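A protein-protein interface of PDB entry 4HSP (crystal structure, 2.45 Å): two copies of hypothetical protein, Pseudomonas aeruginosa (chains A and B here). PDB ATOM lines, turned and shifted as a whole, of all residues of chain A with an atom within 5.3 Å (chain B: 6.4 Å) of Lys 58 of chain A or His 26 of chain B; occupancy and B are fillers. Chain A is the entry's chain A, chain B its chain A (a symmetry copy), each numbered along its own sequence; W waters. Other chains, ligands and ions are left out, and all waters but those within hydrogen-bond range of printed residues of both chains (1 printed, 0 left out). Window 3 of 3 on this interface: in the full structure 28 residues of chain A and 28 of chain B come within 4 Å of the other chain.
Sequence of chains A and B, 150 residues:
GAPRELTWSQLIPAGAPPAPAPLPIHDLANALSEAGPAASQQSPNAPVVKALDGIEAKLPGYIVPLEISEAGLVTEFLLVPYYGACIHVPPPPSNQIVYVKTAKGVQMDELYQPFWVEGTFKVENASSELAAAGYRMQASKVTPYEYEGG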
ATOM      1  N   PRO A   3     -21.886  -6.090 -18.758  1.00  0.00           N
ATOM      2  CA  PRO A   3     -23.297  -5.825 -18.466  1.00  0.00           C
ATOM      3  C   PRO A   3     -24.251  -6.422 -19.500  1.00  0.00           C
ATOM      4  O   PRO A   3     -23.930  -6.488 -20.697  1.00  0.00           O
ATOM      5  CB  PRO A   3     -23.376  -4.302 -18.459  1.00  0.00           C
ATOM      6  CG  PRO A   3     -22.268  -3.870 -19.335  1.00  0.00           C
ATOM      7  CD  PRO A   3     -21.185  -4.872 -19.212  1.00  0.00           C
ATOM      8  N   ARG A   4     -25.431  -6.865 -19.011  1.00  0.00           N
ATOM      9  CA  ARG A   4     -26.568  -7.357 -19.807  1.00  0.00           C
ATOM     10  C   ARG A   4     -27.248  -6.126 -20.371  1.00  0.00           C
ATOM     11  O   ARG A   4     -27.673  -5.276 -19.597  1.00  0.00           O
ATOM     12  CB  ARG A   4     -27.584  -8.171 -18.938  1.00  0.00           C
ATOM     13  CG  ARG A   4     -27.031  -9.431 -18.289  1.00  0.00           C
ATOM     14  CD  ARG A   4     -27.472  -9.683 -16.841  1.00  0.00           C
ATOM     15  NE  ARG A   4     -28.602 -10.617 -16.737  1.00  0.00           N
ATOM     16  CZ  ARG A   4     -28.727 -11.582 -15.825  1.00  0.00           C
ATOM     17  NH1 ARG A   4     -27.770 -11.789 -14.925  1.00  0.00           N
ATOM     18  NH2 ARG A   4     -29.802 -12.362 -15.818  1.00  0.00           N
ATOM     19  N   GLU A   5     -27.325  -5.991 -21.693  1.00  0.00           N
ATOM     20  CA  GLU A   5     -28.031  -4.863 -22.296  1.00  0.00           C
ATOM     21  C   GLU A   5     -29.528  -5.055 -22.120  1.00  0.00           C
ATOM     22  O   GLU A   5     -30.059  -6.124 -22.374  1.00  0.00           O
ATOM     23  CB  GLU A   5     -27.672  -4.673 -23.771  1.00  0.00           C
ATOM     24  CG  GLU A   5     -28.365  -3.463 -24.379  1.00  0.00           C
ATOM     25  CD  GLU A   5     -28.165  -3.203 -25.856  1.00  0.00           C
ATOM     26  OE1 GLU A   5     -27.250  -3.801 -26.465  1.00  0.00           O
ATOM     27  OE2 GLU A   5     -28.910  -2.356 -26.396  1.00  0.00           O
ATOM     28  N   LEU A   6     -30.196  -4.008 -21.681  1.00  0.00           N
ATOM     29  CA  LEU A   6     -31.640  -3.976 -21.497  1.00  0.00           C
ATOM     30  C   LEU A   6     -32.285  -3.015 -22.482  1.00  0.00           C
ATOM     31  O   LEU A   6     -31.618  -2.134 -23.016  1.00  0.00           O
ATOM     32  CB  LEU A   6     -31.989  -3.538 -20.058  1.00  0.00           C
ATOM     33  CG  LEU A   6     -31.502  -4.423 -18.886  1.00  0.00           C
ATOM     34  CD1 LEU A   6     -31.982  -3.830 -17.559  1.00  0.00           C
ATOM     35  CD2 LEU A   6     -31.982  -5.866 -19.034  1.00  0.00           C
ATOM     36  N   GLU A  56     -25.885  -6.862 -13.403  1.00  0.00           N
ATOM     37  CA  GLU A  56     -25.022  -5.847 -14.007  1.00  0.00           C
ATOM     38  C   GLU A  56     -25.722  -5.511 -15.313  1.00  0.00           C
ATOM     39  O   GLU A  56     -25.837  -6.375 -16.175  1.00  0.00           O
ATOM     40  CB  GLU A  56     -23.581  -6.390 -14.203  1.00  0.00           C
ATOM     41  CG  GLU A  56     -22.459  -5.386 -13.973  1.00  0.00           C
ATOM     42  CD  GLU A  56     -22.373  -4.752 -12.592  1.00  0.00           C
ATOM     43  OE1 GLU A  56     -22.733  -5.418 -11.592  1.00  0.00           O
ATOM     44  OE2 GLU A  56     -21.916  -3.587 -12.514  1.00  0.00           O
ATOM     45  N   ALA A  57     -26.304  -4.326 -15.426  1.00  0.00           N
ATOM     46  CA  ALA A  57     -27.099  -3.974 -16.618  1.00  0.00           C
ATOM     47  C   ALA A  57     -26.559  -2.761 -17.371  1.00  0.00           C
ATOM     48  O   ALA A  57     -25.722  -2.033 -16.858  1.00  0.00           O
ATOM     49  CB  ALA A  57     -28.552  -3.735 -16.228  1.00  0.00           C
ATOM     50  N   LYS A  58     -27.043  -2.569 -18.600  1.00  0.00           N
ATOM     51  CA  LYS A  58     -26.680  -1.477 -19.506  1.00  0.00           C
ATOM     52  C   LYS A  58     -27.977  -1.014 -20.185  1.00  0.00           C
ATOM     53  O   LYS A  58     -28.698  -1.806 -20.797  1.00  0.00           O
ATOM     54  CB  LYS A  58     -25.623  -1.982 -20.498  1.00  0.00           C
ATOM     55  CG  LYS A  58     -25.194  -1.028 -21.591  1.00  0.00           C
ATOM     56  CD  LYS A  58     -24.498  -1.843 -22.677  1.00  0.00           C
ATOM     57  CE  LYS A  58     -23.763  -1.003 -23.681  1.00  0.00           C
ATOM     58  NZ  LYS A  58     -23.187  -1.853 -24.750  1.00  0.00           N
ATOM     59  N   LEU A  59     -28.304   0.246 -20.023  1.00  0.00           N
ATOM     60  CA  LEU A  59     -29.547   0.776 -20.568  1.00  0.00           C
ATOM     61  C   LEU A  59     -29.315   2.135 -21.240  1.00  0.00           C
ATOM     62  O   LEU A  59     -28.522   2.925 -20.709  1.00  0.00           O
ATOM     63  CB  LEU A  59     -30.510   0.904 -19.375  1.00  0.00           C
ATOM     64  CG  LEU A  59     -31.992   1.154 -19.572  1.00  0.00           C
ATOM     65  CD1 LEU A  59     -32.663   0.093 -20.454  1.00  0.00           C
ATOM     66  CD2 LEU A  59     -32.662   1.188 -18.208  1.00  0.00           C
ATOM     67  N   PRO A  60     -29.947   2.426 -22.418  1.00  0.00           N
ATOM     68  CA  PRO A  60     -29.769   3.765 -23.029  1.00  0.00           C
ATOM     69  C   PRO A  60     -30.844   4.740 -22.537  1.00  0.00           C
ATOM     70  O   PRO A  60     -31.932   4.325 -22.125  1.00  0.00           O
ATOM     71  CB  PRO A  60     -29.922   3.471 -24.518  1.00  0.00           C
ATOM     72  CG  PRO A  60     -30.937   2.330 -24.548  1.00  0.00           C
ATOM     73  CD  PRO A  60     -30.889   1.607 -23.221  1.00  0.00           C
ATOM     74  N   TRP A 116     -25.406   5.807 -22.558  1.00  0.00           N
ATOM     75  CA  TRP A 116     -25.386   4.424 -22.096  1.00  0.00           C
ATOM     76  C   TRP A 116     -25.021   4.480 -20.604  1.00  0.00           C
ATOM     77  O   TRP A 116     -23.998   5.065 -20.250  1.00  0.00           O
ATOM     78  CB  TRP A 116     -24.366   3.547 -22.876  1.00  0.00           C
ATOM     79  CG  TRP A 116     -24.800   3.174 -24.257  1.00  0.00           C
ATOM     80  CD1 TRP A 116     -24.319   3.670 -25.436  1.00  0.00           C
ATOM     81  CD2 TRP A 116     -25.862   2.277 -24.599  1.00  0.00           C
ATOM     82  NE1 TRP A 116     -25.055   3.180 -26.490  1.00  0.00           N
ATOM     83  CE2 TRP A 116     -26.004   2.313 -26.006  1.00  0.00           C
ATOM     84  CE3 TRP A 116     -26.716   1.445 -23.852  1.00  0.00           C
ATOM     85  CZ2 TRP A 116     -26.936   1.519 -26.681  1.00  0.00           C
ATOM     86  CZ3 TRP A 116     -27.648   0.669 -24.521  1.00  0.00           C
ATOM     87  CH2 TRP A 116     -27.778   0.735 -25.915  1.00  0.00           C
ATOM     88  N   VAL A 117     -25.891   3.958 -19.733  1.00  0.00           N
ATOM     89  CA  VAL A 117     -25.609   3.870 -18.295  1.00  0.00           C
ATOM     90  C   VAL A 117     -25.419   2.368 -17.945  1.00  0.00           C
ATOM     91  O   VAL A 117     -26.359   1.584 -18.072  1.00  0.00           O
ATOM     92  CB  VAL A 117     -26.677   4.544 -17.383  1.00  0.00           C
ATOM     93  CG1 VAL A 117     -26.313   4.351 -15.918  1.00  0.00           C
ATOM     94  CG2 VAL A 117     -26.855   6.025 -17.706  1.00  0.00           C
ATOM     95  N   GLU A 118     -24.217   1.992 -17.518  1.00  0.00           N
ATOM     96  CA  GLU A 118     -23.856   0.638 -17.082  1.00  0.00           C
ATOM     97  C   GLU A 118     -23.623   0.632 -15.598  1.00  0.00           C
ATOM     98  O   GLU A 118     -22.970   1.544 -15.087  1.00  0.00           O
ATOM     99  CB  GLU A 118     -22.556   0.156 -17.774  1.00  0.00           C
ATOM    100  CG  GLU A 118     -22.567   0.242 -19.291  1.00  0.00           C
ATOM    101  CD  GLU A 118     -21.269  -0.124 -19.982  1.00  0.00           C
ATOM    102  OE1 GLU A 118     -20.468  -0.876 -19.382  1.00  0.00           O
ATOM    103  OE2 GLU A 118     -21.065   0.318 -21.137  1.00  0.00           O
ATOM    104  N   GLY A 119     -24.038  -0.431 -14.924  1.00  0.00           N
ATOM    105  CA  GLY A 119     -23.781  -0.580 -13.491  1.00  0.00           C
ATOM    106  C   GLY A 119     -24.629  -1.623 -12.806  1.00  0.00           C
ATOM    107  O   GLY A 119     -25.339  -2.362 -13.467  1.00  0.00           O
ATOM    108  N   MET A 137     -29.796   2.284  -9.893  1.00  0.00           N
ATOM    109  CA  MET A 137     -28.535   1.885 -10.500  1.00  0.00           C
ATOM    110  C   MET A 137     -27.370   2.678  -9.902  1.00  0.00           C
ATOM    111  O   MET A 137     -27.441   3.897  -9.721  1.00  0.00           O
ATOM    112  CB  MET A 137     -28.606   2.082 -12.015  1.00  0.00           C
ATOM    113  CG  MET A 137     -27.430   1.558 -12.807  1.00  0.00           C
ATOM    114  SD  MET A 137     -28.055   1.161 -14.631  1.00  0.00           S
ATOM    115  CE  MET A 137     -27.628  -0.616 -14.610  1.00  0.00           C
ATOM    116  N   PRO B  24     -32.613   2.718 -30.400  1.00  0.00           N
ATOM    117  CA  PRO B  24     -32.223   1.363 -30.840  1.00  0.00           C
ATOM    118  C   PRO B  24     -31.189   0.657 -29.961  1.00  0.00           C
ATOM    119  O   PRO B  24     -30.334   1.290 -29.364  1.00  0.00           O
ATOM    120  CB  PRO B  24     -31.602   1.596 -32.223  1.00  0.00           C
ATOM    121  CG  PRO B  24     -32.060   2.871 -32.652  1.00  0.00           C
ATOM    122  CD  PRO B  24     -32.402   3.707 -31.474  1.00  0.00           C
ATOM    123  N   ILE B  25     -31.221  -0.670 -29.967  1.00  0.00           N
ATOM    124  CA  ILE B  25     -30.239  -1.492 -29.274  1.00  0.00           C
ATOM    125  C   ILE B  25     -28.866  -1.194 -29.877  1.00  0.00           C
ATOM    126  O   ILE B  25     -28.776  -0.767 -31.039  1.00  0.00           O
ATOM    127  CB  ILE B  25     -30.584  -2.996 -29.304  1.00  0.00           C
ATOM    128  CG1 ILE B  25     -30.776  -3.513 -30.737  1.00  0.00           C
ATOM    129  CG2 ILE B  25     -31.795  -3.287 -28.404  1.00  0.00           C
ATOM    130  CD1 ILE B  25     -30.539  -5.068 -30.891  1.00  0.00           C
ATOM    131  N   HIS B  26     -27.833  -1.347 -29.064  1.00  0.00           N
ATOM    132  CA  HIS B  26     -26.445  -1.045 -29.379  1.00  0.00           C
ATOM    133  C   HIS B  26     -25.971  -1.644 -30.705  1.00  0.00           C
ATOM    134  O   HIS B  26     -25.384  -0.933 -31.518  1.00  0.00           O
ATOM    135  CB  HIS B  26     -25.554  -1.543 -28.239  1.00  0.00           C
ATOM    136  CG  HIS B  26     -24.106  -1.292 -28.459  1.00  0.00           C
ATOM    137  ND1 HIS B  26     -23.547  -0.056 -28.202  1.00  0.00           N
ATOM    138  CD2 HIS B  26     -23.135  -2.144 -28.870  1.00  0.00           C
ATOM    139  CE1 HIS B  26     -22.253  -0.190 -28.448  1.00  0.00           C
ATOM    140  NE2 HIS B  26     -21.963  -1.428 -28.881  1.00  0.00           N
ATOM    141  N   ASP B  27     -26.206  -2.936 -30.915  1.00  0.00           N
ATOM    142  CA  ASP B  27     -25.757  -3.587 -32.137  1.00  0.00           C
ATOM    143  C   ASP B  27     -26.427  -2.984 -33.388  1.00  0.00           C
ATOM    144  O   ASP B  27     -25.745  -2.791 -34.384  1.00  0.00           O
ATOM    145  CB  ASP B  27     -25.968  -5.094 -32.039  1.00  0.00           C
ATOM    146  CG  ASP B  27     -25.035  -5.772 -31.039  1.00  0.00           C
ATOM    147  OD1 ASP B  27     -24.048  -5.118 -30.590  1.00  0.00           O
ATOM    148  OD2 ASP B  27     -25.264  -6.964 -30.731  1.00  0.00           O
ATOM    149  N   LEU B  28     -27.713  -2.600 -33.288  1.00  0.00           N
ATOM    150  CA  LEU B  28     -28.478  -1.973 -34.357  1.00  0.00           C
ATOM    151  C   LEU B  28     -27.977  -0.540 -34.645  1.00  0.00           C
ATOM    152  O   LEU B  28     -27.828  -0.194 -35.810  1.00  0.00           O
ATOM    153  CB  LEU B  28     -29.993  -1.968 -34.040  1.00  0.00           C
ATOM    154  CG  LEU B  28     -30.954  -1.334 -35.097  1.00  0.00           C
ATOM    155  CD1 LEU B  28     -30.814  -1.984 -36.505  1.00  0.00           C
ATOM    156  CD2 LEU B  28     -32.383  -1.414 -34.632  1.00  0.00           C
ATOM    157  N   ALA B  29     -27.773   0.290 -33.619  1.00  0.00           N
ATOM    158  CA  ALA B  29     -27.252   1.652 -33.786  1.00  0.00           C
ATOM    159  C   ALA B  29     -25.857   1.599 -34.449  1.00  0.00           C
ATOM    160  O   ALA B  29     -25.586   2.400 -35.349  1.00  0.00           O
ATOM    161  CB  ALA B  29     -27.181   2.365 -32.442  1.00  0.00           C
ATOM    162  N   ASN B  30     -25.001   0.621 -34.042  1.00  0.00           N
ATOM    163  CA  ASN B  30     -23.695   0.433 -34.652  1.00  0.00           C
ATOM    164  C   ASN B  30     -23.836  -0.044 -36.094  1.00  0.00           C
ATOM    165  O   ASN B  30     -23.107   0.464 -36.943  1.00  0.00           O
ATOM    166  CB  ASN B  30     -22.801  -0.526 -33.854  1.00  0.00           C
ATOM    167  CG  ASN B  30     -22.112   0.114 -32.663  1.00  0.00           C
ATOM    168  OD1 ASN B  30     -22.250   1.319 -32.376  1.00  0.00           O
ATOM    169  ND2 ASN B  30     -21.404  -0.702 -31.899  1.00  0.00           N
ATOM    170  N   ALA B  31     -24.794  -0.966 -36.386  1.00  0.00           N
ATOM    171  CA  ALA B  31     -24.996  -1.462 -37.748  1.00  0.00           C
ATOM    172  C   ALA B  31     -25.434  -0.354 -38.700  1.00  0.00           C
ATOM    173  O   ALA B  31     -24.954  -0.327 -39.819  1.00  0.00           O
ATOM    174  CB  ALA B  31     -25.999  -2.600 -37.773  1.00  0.00           C
HETATM  175  O   HOH W   1     -27.216  -4.769 -28.923  1.00  0.00           O
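The backbone NH (N) of His 26 of chain B sits at hydrogen-bond distance from the side-chain carboxylate (OE2) of Glu 5 of chain A (3.0 Å).
The backbone NH (N) of Lys 58 of chain A is in hydrogen-bond range of the backbone carbonyl oxygen (O) of Arg 4 of chain A (3.0 Å). A ring nitrogen (NE2) of His 26 of chain B sits at hydrogen-bond distance from the side-chain amide nitrogen (ND2) of Asn 30 of chain B (3.2 Å). N of Leu 6 of chain A lies within hydrogen-bond range of O of Lys 58 of chain A, at 2.8 Å.
Among the printed residues, pairs that only touch across the chains: Glu 5 of chain A with Ile 25 of chain B (3.3 Å), Lys 58 of chain A with His 26 of chain B (3.9 Å) and Trp 116 of chain A with His 26 of chain B (3.7 Å).
Of the printed residues of chain B, Glu 5 of chain A touches Ile 25 and His 26. Lys 58 of chain A touches just one residue of chain B: His 26 (3.9 Å). Printed residues of chain B within 4 Å of Trp 116 of chain A: His 26. Of the printed residues of chain A, Ile 25 of chain B touches Glu 5 (3.3 Å). Of the printed residues of chain A, His 26 of chain B touches Glu 5 (3.0 Å), Lys 58 (3.9 Å) and Trp 116 (3.7 Å). The nearest printed residue of chain B that does not touch Lys 58 of chain A is Asp 27 of chain B (6.7 Å). The nearest printed residue of chain A that does not touch Ile 25 of chain B is Trp 116 of chain A (4.5 Å).
Printed residues of chain A that touch a printed residue of chain B: Glu 5, Lys 58 and Trp 116. Among the printed residues, 4 pairs touch across the chains. Among the printed residues, no Asp or Glu carboxylate lies within 4 Å of a Lys or Arg side-chain nitrogen of the other chain.
No position is printed for both chains.
Water W1 lies within hydrogen-bond range of the side-chain carboxylate of Glu 5 of chain A (2.6 Å), the backbone NH of Asp 27 of chain B (2.9 Å) and the backbone NH of His 26 of chain B (3.5 Å).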
